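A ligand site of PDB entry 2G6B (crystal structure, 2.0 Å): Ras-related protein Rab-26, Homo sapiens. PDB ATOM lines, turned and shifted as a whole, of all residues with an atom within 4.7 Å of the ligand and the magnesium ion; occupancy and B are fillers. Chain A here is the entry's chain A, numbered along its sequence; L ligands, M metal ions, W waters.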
ATOM      1  N   GLY A  17      28.050   8.794 -27.534  1.00  0.00           N
ATOM      2  CA  GLY A  17      29.376   8.794 -26.958  1.00  0.00           C
ATOM      3  C   GLY A  17      30.128   7.538 -27.391  1.00  0.00           C
ATOM      4  O   GLY A  17      29.522   6.606 -27.928  1.00  0.00           O
ATOM      5  N   ASP A  18      31.431   7.534 -27.171  1.00  0.00           N
ATOM      6  CA  ASP A  18      32.314   6.421 -27.587  1.00  0.00           C
ATOM      7  C   ASP A  18      31.863   5.080 -27.030  1.00  0.00           C
ATOM      8  O   ASP A  18      31.247   5.005 -25.989  1.00  0.00           O
ATOM      9  CB  ASP A  18      33.753   6.670 -27.120  1.00  0.00           C
ATOM     10  CG  ASP A  18      34.486   7.708 -27.971  1.00  0.00           C
ATOM     11  OD1 ASP A  18      33.849   8.362 -28.805  1.00  0.00           O
ATOM     12  OD2 ASP A  18      35.696   7.865 -27.789  1.00  0.00           O
ATOM     13  N   SER A  19      32.215   4.028 -27.723  1.00  0.00           N
ATOM     14  CA  SER A  19      31.909   2.730 -27.246  1.00  0.00           C
ATOM     15  C   SER A  19      32.621   2.528 -25.929  1.00  0.00           C
ATOM     16  O   SER A  19      33.769   2.853 -25.786  1.00  0.00           O
ATOM     17  CB  SER A  19      32.361   1.665 -28.232  1.00  0.00           C
ATOM     18  OG  SER A  19      32.120   0.400 -27.681  1.00  0.00           O
ATOM     19  N   GLY A  20      31.911   1.981 -24.964  1.00  0.00           N
ATOM     20  CA  GLY A  20      32.482   1.662 -23.690  1.00  0.00           C
ATOM     21  C   GLY A  20      32.274   2.708 -22.609  1.00  0.00           C
ATOM     22  O   GLY A  20      32.622   2.472 -21.446  1.00  0.00           O
ATOM     23  N   VAL A  21      31.730   3.858 -22.957  1.00  0.00           N
ATOM     24  CA  VAL A  21      31.659   4.925 -21.947  1.00  0.00           C
ATOM     25  C   VAL A  21      30.583   4.694 -20.865  1.00  0.00           C
ATOM     26  O   VAL A  21      30.640   5.333 -19.783  1.00  0.00           O
ATOM     27  CB  VAL A  21      31.501   6.332 -22.576  1.00  0.00           C
ATOM     28  CG1 VAL A  21      32.736   6.662 -23.459  1.00  0.00           C
ATOM     29  CG2 VAL A  21      30.189   6.409 -23.319  1.00  0.00           C
ATOM     30  N   GLY A  22      29.609   3.833 -21.160  1.00  0.00           N
ATOM     31  CA  GLY A  22      28.562   3.534 -20.182  1.00  0.00           C
ATOM     32  C   GLY A  22      27.147   3.900 -20.539  1.00  0.00           C
ATOM     33  O   GLY A  22      26.308   3.924 -19.652  1.00  0.00           O
ATOM     34  N   LYS A  23      26.867   4.157 -21.828  1.00  0.00           N
ATOM     35  CA  LYS A  23      25.500   4.539 -22.307  1.00  0.00           C
ATOM     36  C   LYS A  23      24.419   3.520 -21.893  1.00  0.00           C
ATOM     37  O   LYS A  23      23.417   3.885 -21.233  1.00  0.00           O
ATOM     38  CB  LYS A  23      25.489   4.733 -23.840  1.00  0.00           C
ATOM     39  CG  LYS A  23      26.433   5.846 -24.337  1.00  0.00           C
ATOM     40  CD  LYS A  23      26.393   6.015 -25.859  1.00  0.00           C
ATOM     41  CE  LYS A  23      26.972   4.806 -26.627  1.00  0.00           C
ATOM     42  NZ  LYS A  23      28.336   4.465 -26.235  1.00  0.00           N
ATOM     43  N   THR A  24      24.626   2.259 -22.246  1.00  0.00           N
ATOM     44  CA  THR A  24      23.680   1.179 -21.899  1.00  0.00           C
ATOM     45  C   THR A  24      23.497   1.026 -20.370  1.00  0.00           C
ATOM     46  O   THR A  24      22.366   1.039 -19.835  1.00  0.00           O
ATOM     47  CB  THR A  24      24.085  -0.209 -22.561  1.00  0.00           C
ATOM     48  OG1 THR A  24      24.240  -0.026 -23.964  1.00  0.00           O
ATOM     49  CG2 THR A  24      23.035  -1.260 -22.314  1.00  0.00           C
ATOM     50  N   CYS A  25      24.603   0.943 -19.653  1.00  0.00           N
ATOM     51  CA  CYS A  25      24.535   0.858 -18.194  1.00  0.00           C
ATOM     52  C   CYS A  25      23.887   2.049 -17.532  1.00  0.00           C
ATOM     53  O   CYS A  25      23.179   1.887 -16.540  1.00  0.00           O
ATOM     54  CB  CYS A  25      25.925   0.621 -17.565  1.00  0.00           C
ATOM     55  SG  CYS A  25      26.507  -0.987 -17.872  1.00  0.00           S
ATOM     56  N   PHE A  35      22.785  -1.707 -11.201  1.00  0.00           N
ATOM     57  CA  PHE A  35      23.987  -1.850 -12.013  1.00  0.00           C
ATOM     58  C   PHE A  35      24.297  -3.319 -12.028  1.00  0.00           C
ATOM     59  O   PHE A  35      24.579  -3.921 -10.977  1.00  0.00           O
ATOM     60  CB  PHE A  35      25.149  -1.129 -11.395  1.00  0.00           C
ATOM     61  CG  PHE A  35      26.445  -1.315 -12.131  1.00  0.00           C
ATOM     62  CD1 PHE A  35      26.657  -0.692 -13.385  1.00  0.00           C
ATOM     63  CD2 PHE A  35      27.472  -2.081 -11.572  1.00  0.00           C
ATOM     64  CE1 PHE A  35      27.838  -0.854 -14.056  1.00  0.00           C
ATOM     65  CE2 PHE A  35      28.664  -2.250 -12.239  1.00  0.00           C
ATOM     66  CZ  PHE A  35      28.864  -1.629 -13.486  1.00  0.00           C
ATOM     67  N   LEU A  36      24.228  -3.910 -13.210  1.00  0.00           N
ATOM     68  CA  LEU A  36      24.617  -5.286 -13.371  1.00  0.00           C
ATOM     69  C   LEU A  36      26.069  -5.262 -13.820  1.00  0.00           C
ATOM     70  O   LEU A  36      26.396  -4.750 -14.913  1.00  0.00           O
ATOM     71  CB  LEU A  36      23.717  -5.988 -14.408  1.00  0.00           C
ATOM     72  N   PHE A  40      30.155  -7.231 -20.755  1.00  0.00           N
ATOM     73  CA  PHE A  40      30.187  -6.066 -21.616  1.00  0.00           C
ATOM     74  C   PHE A  40      29.629  -6.464 -22.972  1.00  0.00           C
ATOM     75  O   PHE A  40      30.260  -7.184 -23.712  1.00  0.00           O
ATOM     76  CB  PHE A  40      31.583  -5.479 -21.801  1.00  0.00           C
ATOM     77  CG  PHE A  40      31.629  -4.374 -22.855  1.00  0.00           C
ATOM     78  CD1 PHE A  40      30.571  -3.453 -22.977  1.00  0.00           C
ATOM     79  CD2 PHE A  40      32.718  -4.247 -23.696  1.00  0.00           C
ATOM     80  CE1 PHE A  40      30.605  -2.422 -23.937  1.00  0.00           C
ATOM     81  CE2 PHE A  40      32.772  -3.202 -24.661  1.00  0.00           C
ATOM     82  CZ  PHE A  40      31.703  -2.292 -24.775  1.00  0.00           C
ATOM     83  N   ILE A  41      28.425  -6.003 -23.251  1.00  0.00           N
ATOM     84  CA  ILE A  41      27.779  -6.255 -24.517  1.00  0.00           C
ATOM     85  C   ILE A  41      27.617  -4.947 -25.291  1.00  0.00           C
ATOM     86  O   ILE A  41      26.715  -4.129 -24.986  1.00  0.00           O
ATOM     87  CB  ILE A  41      26.432  -6.932 -24.312  1.00  0.00           C
ATOM     88  CG1 ILE A  41      26.650  -8.313 -23.653  1.00  0.00           C
ATOM     89  CG2 ILE A  41      25.722  -7.039 -25.626  1.00  0.00           C
ATOM     90  CD1 ILE A  41      25.389  -9.019 -23.228  1.00  0.00           C
ATOM     91  N   SER A  42      28.489  -4.736 -26.261  1.00  0.00           N
ATOM     92  CA  SER A  42      28.445  -3.594 -27.169  1.00  0.00           C
ATOM     93  C   SER A  42      27.166  -3.537 -27.964  1.00  0.00           C
ATOM     94  O   SER A  42      26.781  -4.497 -28.626  1.00  0.00           O
ATOM     95  CB  SER A  42      29.603  -3.600 -28.149  1.00  0.00           C
ATOM     96  OG  SER A  42      30.603  -2.691 -27.742  1.00  0.00           O
ATOM     97  N   THR A  43      26.520  -2.369 -27.882  1.00  0.00           N
ATOM     98  CA  THR A  43      25.237  -2.092 -28.539  1.00  0.00           C
ATOM     99  C   THR A  43      25.436  -1.981 -30.019  1.00  0.00           C
ATOM    100  O   THR A  43      26.317  -1.255 -30.458  1.00  0.00           O
ATOM    101  CB  THR A  43      24.651  -0.755 -27.979  1.00  0.00           C
ATOM    102  OG1 THR A  43      24.668  -0.849 -26.575  1.00  0.00           O
ATOM    103  CG2 THR A  43      23.182  -0.486 -28.457  1.00  0.00           C
ATOM    104  N   ASP A  66      19.115   4.249 -26.732  1.00  0.00           N
ATOM    105  CA  ASP A  66      20.490   3.812 -26.660  1.00  0.00           C
ATOM    106  C   ASP A  66      21.021   3.733 -28.083  1.00  0.00           C
ATOM    107  O   ASP A  66      20.264   3.549 -28.998  1.00  0.00           O
ATOM    108  CB  ASP A  66      20.555   2.432 -26.064  1.00  0.00           C
ATOM    109  CG  ASP A  66      21.851   2.121 -25.453  1.00  0.00           C
ATOM    110  OD1 ASP A  66      22.781   2.986 -25.490  1.00  0.00           O
ATOM    111  OD2 ASP A  66      21.956   0.992 -24.907  1.00  0.00           O
ATOM    112  N   THR A  67      22.316   3.870 -28.242  1.00  0.00           N
ATOM    113  CA  THR A  67      22.917   3.890 -29.560  1.00  0.00           C
ATOM    114  C   THR A  67      24.263   3.176 -29.518  1.00  0.00           C
ATOM    115  O   THR A  67      24.858   3.021 -28.476  1.00  0.00           O
ATOM    116  CB  THR A  67      23.125   5.327 -30.077  1.00  0.00           C
ATOM    117  OG1 THR A  67      24.086   5.987 -29.260  1.00  0.00           O
ATOM    118  CG2 THR A  67      21.815   6.143 -30.110  1.00  0.00           C
ATOM    119  N   ALA A  68      24.745   2.796 -30.692  1.00  0.00           N
ATOM    120  CA  ALA A  68      26.026   2.149 -30.834  1.00  0.00           C
ATOM    121  C   ALA A  68      27.148   3.200 -30.771  1.00  0.00           C
ATOM    122  O   ALA A  68      27.091   4.200 -31.465  1.00  0.00           O
ATOM    123  CB  ALA A  68      26.058   1.397 -32.166  1.00  0.00           C
ATOM    124  N   GLY A  69      28.164   2.968 -29.931  1.00  0.00           N
ATOM    125  CA  GLY A  69      29.333   3.871 -29.899  1.00  0.00           C
ATOM    126  C   GLY A  69      30.433   3.482 -30.873  1.00  0.00           C
ATOM    127  O   GLY A  69      31.277   4.314 -31.213  1.00  0.00           O
ATOM    128  N   GLN A  70      30.452   2.222 -31.312  1.00  0.00           N
ATOM    129  CA  GLN A  70      31.473   1.717 -32.255  1.00  0.00           C
ATOM    130  C   GLN A  70      31.218   2.198 -33.693  1.00  0.00           C
ATOM    131  O   GLN A  70      30.064   2.113 -34.165  1.00  0.00           O
ATOM    132  CB  GLN A  70      31.561   0.187 -32.205  1.00  0.00           C
ATOM    133  CG  GLN A  70      31.983  -0.339 -30.846  1.00  0.00           C
ATOM    134  CD  GLN A  70      32.619  -1.727 -30.860  1.00  0.00           C
ATOM    135  OE1 GLN A  70      32.046  -2.688 -31.342  1.00  0.00           O
ATOM    136  NE2 GLN A  70      33.823  -1.823 -30.268  1.00  0.00           N
ATOM    137  N   ASN A 124      31.158  10.019 -17.020  1.00  0.00           N
ATOM    138  CA  ASN A 124      30.706   8.826 -16.343  1.00  0.00           C
ATOM    139  C   ASN A 124      31.879   7.999 -15.784  1.00  0.00           C
ATOM    140  O   ASN A 124      33.045   8.289 -16.066  1.00  0.00           O
ATOM    141  CB  ASN A 124      29.839   8.003 -17.322  1.00  0.00           C
ATOM    142  CG  ASN A 124      29.106   6.853 -16.646  1.00  0.00           C
ATOM    143  OD1 ASN A 124      28.452   7.035 -15.618  1.00  0.00           O
ATOM    144  ND2 ASN A 124      29.223   5.671 -17.213  1.00  0.00           N
ATOM    145  N   LYS A 125      31.541   6.986 -15.002  1.00  0.00           N
ATOM    146  CA  LYS A 125      32.499   6.079 -14.291  1.00  0.00           C
ATOM    147  C   LYS A 125      33.280   6.784 -13.188  1.00  0.00           C
ATOM    148  O   LYS A 125      34.438   6.464 -12.941  1.00  0.00           O
ATOM    149  CB  LYS A 125      33.446   5.349 -15.261  1.00  0.00           C
ATOM    150  CG  LYS A 125      32.705   4.656 -16.424  1.00  0.00           C
ATOM    151  CD  LYS A 125      33.437   3.442 -16.898  1.00  0.00           C
ATOM    152  CE  LYS A 125      33.081   3.095 -18.283  1.00  0.00           C
ATOM    153  NZ  LYS A 125      33.785   1.861 -18.786  1.00  0.00           N
ATOM    154  N   ASP A 127      33.841   6.524  -9.923  1.00  0.00           N
ATOM    155  CA  ASP A 127      33.705   5.536  -8.851  1.00  0.00           C
ATOM    156  C   ASP A 127      35.057   4.807  -8.585  1.00  0.00           C
ATOM    157  O   ASP A 127      36.042   5.051  -9.296  1.00  0.00           O
ATOM    158  CB  ASP A 127      32.543   4.541  -9.162  1.00  0.00           C
ATOM    159  CG  ASP A 127      32.681   3.872 -10.515  1.00  0.00           C
ATOM    160  OD1 ASP A 127      33.641   3.074 -10.653  1.00  0.00           O
ATOM    161  OD2 ASP A 127      31.848   4.133 -11.442  1.00  0.00           O
ATOM    162  N   ALA A 129      36.188   1.871  -9.212  1.00  0.00           N
ATOM    163  CA  ALA A 129      36.595   0.824 -10.141  1.00  0.00           C
ATOM    164  C   ALA A 129      37.902   1.100 -10.903  1.00  0.00           C
ATOM    165  O   ALA A 129      38.775   0.232 -10.952  1.00  0.00           O
ATOM    166  CB  ALA A 129      35.462   0.551 -11.127  1.00  0.00           C
ATOM    167  N   HIS A 130      38.036   2.286 -11.498  1.00  0.00           N
ATOM    168  CA  HIS A 130      39.216   2.625 -12.284  1.00  0.00           C
ATOM    169  C   HIS A 130      39.727   4.022 -11.915  1.00  0.00           C
ATOM    170  O   HIS A 130      39.039   4.814 -11.251  1.00  0.00           O
ATOM    171  CB  HIS A 130      38.930   2.569 -13.774  1.00  0.00           C
ATOM    172  CG  HIS A 130      38.044   1.426 -14.186  1.00  0.00           C
ATOM    173  ND1 HIS A 130      38.546   0.166 -14.451  1.00  0.00           N
ATOM    174  CD2 HIS A 130      36.713   1.363 -14.402  1.00  0.00           C
ATOM    175  CE1 HIS A 130      37.542  -0.635 -14.800  1.00  0.00           C
ATOM    176  NE2 HIS A 130      36.423   0.066 -14.765  1.00  0.00           N
ATOM    177  N   SER A 154      27.887   7.914 -12.337  1.00  0.00           N
ATOM    178  CA  SER A 154      28.280   6.519 -12.231  1.00  0.00           C
ATOM    179  C   SER A 154      27.059   5.629 -12.313  1.00  0.00           C
ATOM    180  O   SER A 154      26.180   5.673 -11.450  1.00  0.00           O
ATOM    181  CB  SER A 154      29.018   6.238 -10.934  1.00  0.00           C
ATOM    182  OG  SER A 154      29.215   4.835 -10.788  1.00  0.00           O
ATOM    183  N   ALA A 155      27.018   4.782 -13.349  1.00  0.00           N
ATOM    184  CA  ALA A 155      25.981   3.727 -13.435  1.00  0.00           C
ATOM    185  C   ALA A 155      26.179   2.727 -12.281  1.00  0.00           C
ATOM    186  O   ALA A 155      25.213   2.191 -11.731  1.00  0.00           O
ATOM    187  CB  ALA A 155      26.052   2.990 -14.797  1.00  0.00           C
ATOM    188  N   LYS A 156      27.429   2.527 -11.881  1.00  0.00           N
ATOM    189  CA  LYS A 156      27.758   1.587 -10.812  1.00  0.00           C
ATOM    190  C   LYS A 156      27.192   1.992  -9.435  1.00  0.00           C
ATOM    191  O   LYS A 156      26.515   1.201  -8.776  1.00  0.00           O
ATOM    192  CB  LYS A 156      29.267   1.340 -10.766  1.00  0.00           C
ATOM    193  CG  LYS A 156      29.695   0.202  -9.813  1.00  0.00           C
ATOM    194  CD  LYS A 156      31.214   0.043  -9.735  1.00  0.00           C
ATOM    195  CE  LYS A 156      31.622  -1.204  -8.901  1.00  0.00           C
ATOM    196  NZ  LYS A 156      31.914  -2.434  -9.767  1.00  0.00           N
HETATM  197  P1  LIG L   1      28.666   0.692 -26.550  1.00  0.00           P
HETATM  198  O1  LIG L   1      29.734  -0.177 -27.157  1.00  0.00           O
HETATM  199  O2  LIG L   1      27.309  -0.012 -26.559  1.00  0.00           O
HETATM  200  O3  LIG L   1      28.650   2.063 -27.225  1.00  0.00           O
HETATM  201  N1  LIG L   1      29.145   0.848 -24.999  1.00  0.00           N
HETATM  202  P2  LIG L   1      28.346   1.623 -23.823  1.00  0.00           P
HETATM  203  O4  LIG L   1      28.647   3.071 -23.875  1.00  0.00           O
HETATM  204  O5  LIG L   1      26.938   1.220 -23.808  1.00  0.00           O
HETATM  205  O6  LIG L   1      28.932   1.100 -22.472  1.00  0.00           O
HETATM  206  P3  LIG L   1      28.352   0.007 -21.482  1.00  0.00           P
HETATM  207  O7  LIG L   1      27.232   0.523 -20.710  1.00  0.00           O
HETATM  208  O8  LIG L   1      28.218  -1.295 -22.183  1.00  0.00           O
HETATM  209  O9  LIG L   1      29.475  -0.134 -20.409  1.00  0.00           O
HETATM  210  C1  LIG L   1      30.848  -0.407 -20.788  1.00  0.00           C
HETATM  211  C2  LIG L   1      31.609  -1.127 -19.687  1.00  0.00           C
HETATM  212  O10 LIG L   1      31.844  -0.227 -18.556  1.00  0.00           O
HETATM  213  C3  LIG L   1      30.903  -2.332 -19.085  1.00  0.00           C
HETATM  214  O11 LIG L   1      31.841  -3.325 -18.642  1.00  0.00           O
HETATM  215  C4  LIG L   1      30.130  -1.737 -17.913  1.00  0.00           C
HETATM  216  O12 LIG L   1      29.863  -2.643 -16.868  1.00  0.00           O
HETATM  217  C5  LIG L   1      31.119  -0.708 -17.430  1.00  0.00           C
HETATM  218  N2  LIG L   1      30.519   0.494 -16.858  1.00  0.00           N
HETATM  219  C6  LIG L   1      29.546   1.284 -17.400  1.00  0.00           C
HETATM  220  N3  LIG L   1      29.251   2.309 -16.696  1.00  0.00           N
HETATM  221  C7  LIG L   1      30.135   2.209 -15.621  1.00  0.00           C
HETATM  222  C8  LIG L   1      30.295   3.049 -14.513  1.00  0.00           C
HETATM  223  O13 LIG L   1      29.667   4.080 -14.218  1.00  0.00           O
HETATM  224  N4  LIG L   1      31.273   2.573 -13.665  1.00  0.00           N
HETATM  225  C9  LIG L   1      32.012   1.434 -13.854  1.00  0.00           C
HETATM  226  N5  LIG L   1      32.904   1.199 -12.898  1.00  0.00           N
HETATM  227  N6  LIG L   1      31.892   0.623 -14.876  1.00  0.00           N
HETATM  228  C10 LIG L   1      30.925   1.092 -15.720  1.00  0.00           C
HETATM  229 MG    MG M   1      25.878   0.088 -25.146  1.00  0.00          MG
HETATM  230  O   HOH W   1      26.429  -1.550 -24.216  1.00  0.00           O
HETATM  231  O   HOH W   2      31.619  -3.412 -15.099  1.00  0.00           O
HETATM  232  O   HOH W   3      27.459  -3.835 -21.185  1.00  0.00           O
HETATM  233  O   HOH W   4      27.952  -4.503 -18.486  1.00  0.00           O
HETATM  234  O   HOH W   5      28.647  -0.038 -29.951  1.00  0.00           O
HETATM  235  O   HOH W   6      34.769   0.212 -16.959  1.00  0.00           O
HETATM  236  O   HOH W   7      25.197   1.806 -26.039  1.00  0.00           O
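The backbone NH of Thr 43 lies close to an oxygen (O2) of the ligand (2.8 Å).
The side-chain carboxylate (OD2) of Asp 127 sits at hydrogen-bond distance from a nitrogen (N4) of the ligand (2.8 Å).
The side-chain sulfur of Cys 25 is in hydrogen-bond range of an oxygen (O7) of the ligand (3.3 Å).
N of Cys 25 lies within hydrogen-bond range of O7 of the ligand, at 2.9 Å.
NZ of Lys 125 is in hydrogen-bond range of O10 of the ligand (2.9 Å).
The backbone NH (N) of Thr 24 sits at hydrogen-bond distance from an oxygen (O7) of the ligand (3.5 Å).
O4 of the ligand lies within hydrogen-bond range of N of Lys 23 (2.9 Å).
N of Gly 69 lies within hydrogen-bond range of O3 of the ligand (2.9 Å).
An oxygen (O1) of the ligand lies within hydrogen-bond range of the side-chain hydroxyl (OG) of Ser 42 (2.7 Å).
The side-chain amino group (NZ) of Lys 23 lies within salt-bridge range of an oxygen (O3) of the ligand.
N of Gly 22 sits at hydrogen-bond distance from O4 of the ligand (3.0 Å).
The side-chain amide nitrogen (ND2) of Asn 124 is in hydrogen-bond range of a nitrogen (N3) of the ligand (3.4 Å).
An oxygen (O4) of the ligand lies within hydrogen-bond range of the backbone NH (N) of Val 21.
O13 of the ligand sits at hydrogen-bond distance from N of Ala 155 (2.9 Å).
OG of Ser 19 sits at hydrogen-bond distance from O1 of the ligand (2.5 Å).
The backbone NH (N) of Ala 129 lies close to the side-chain carboxylate (OD1) of Asp 127 (3.2 Å).
OD1 of Asn 124 sits close to N of Ser 154.
The side-chain carboxylate (OD2) of Asp 127 sits at hydrogen-bond distance from the side-chain hydroxyl (OG) of Ser 154 (2.8 Å).
OG of Ser 19 is in hydrogen-bond range of OG of Ser 42.
The side-chain amide nitrogen of Asn 124 is in hydrogen-bond range of the backbone carbonyl oxygen of Val 21.
The side-chain amino group (NZ) of Lys 125 lies within hydrogen-bond range of the backbone carbonyl oxygen (O) of Gly 20 (3.0 Å).
NZ of Lys 23 is in hydrogen-bond range of O of Gly 17.
The backbone carbonyl oxygen of Asp 18 is in hydrogen-bond range of the side-chain amino group of Lys 23 (3.0 Å).
The backbone NH (N) of Gly 20 lies close to a nitrogen (N1) of the ligand (3.0 Å).
Merely in contact with the ligand: Phe 40, Ala 129, Ser 154, Lys 156, Phe 35 and Asp 18.
Hydrophobic or aromatic side chains that line the ligand: Val 21, Phe 35, Phe 40, Ala 129 and Ala 155.
20 residues have an atom within 4 Å of the ligand: Asp 18, Ser 19, Gly 20, Val 21, Gly 22, Lys 23, Thr 24, Cys 25, Phe 35, Phe 40, Ser 42, Thr 43, Gly 69, Asn 124, Lys 125, Asp 127, Ala 129, Ser 154, Ala 155 and Lys 156.
The nearest printed residue that does not touch the ligand is Ala 68 (4.02 Å).
Two residues have an atom within 4 Å of the magnesium ion: Thr 24 and Thr 43.
Water W1 binds the magnesium ion (2.0 Å).
The magnesium ion is bound by O2 of the ligand, at 2.0 Å.
OG1 of Thr 24 is bound to the magnesium ion (2.0 Å).
The magnesium ion is bound by O5 of the ligand (2.0 Å).
Water W7 binds the magnesium ion, at 2.1 Å.
The side-chain hydroxyl (OG1) of Thr 43 is bound to the magnesium ion.
The magnesium ion has six donor atoms within binding distance.
Water W7 lies within hydrogen-bond range of the backbone carbonyl oxygen (O) of Thr 67 (2.7 Å) and the side-chain carboxylate (OD1) of Asp 66 (2.7 Å).
Water W1 bridges O of Ile 41 (2.7 Å) and O8 of the ligand (2.7 Å).
Water W3 bridges O8 of the ligand and N of Ile 41.
Water W5 lies within hydrogen-bond range of the backbone carbonyl oxygen of Thr 43, an oxygen (O1) of the ligand, the backbone NH of Gly 69 and the backbone NH of Gln 70.
Water W6 lies within hydrogen-bond range of the side-chain amino group (NZ) of Lys 125, a ring nitrogen (NE2) of His 130 and an oxygen (O10) of the ligand.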
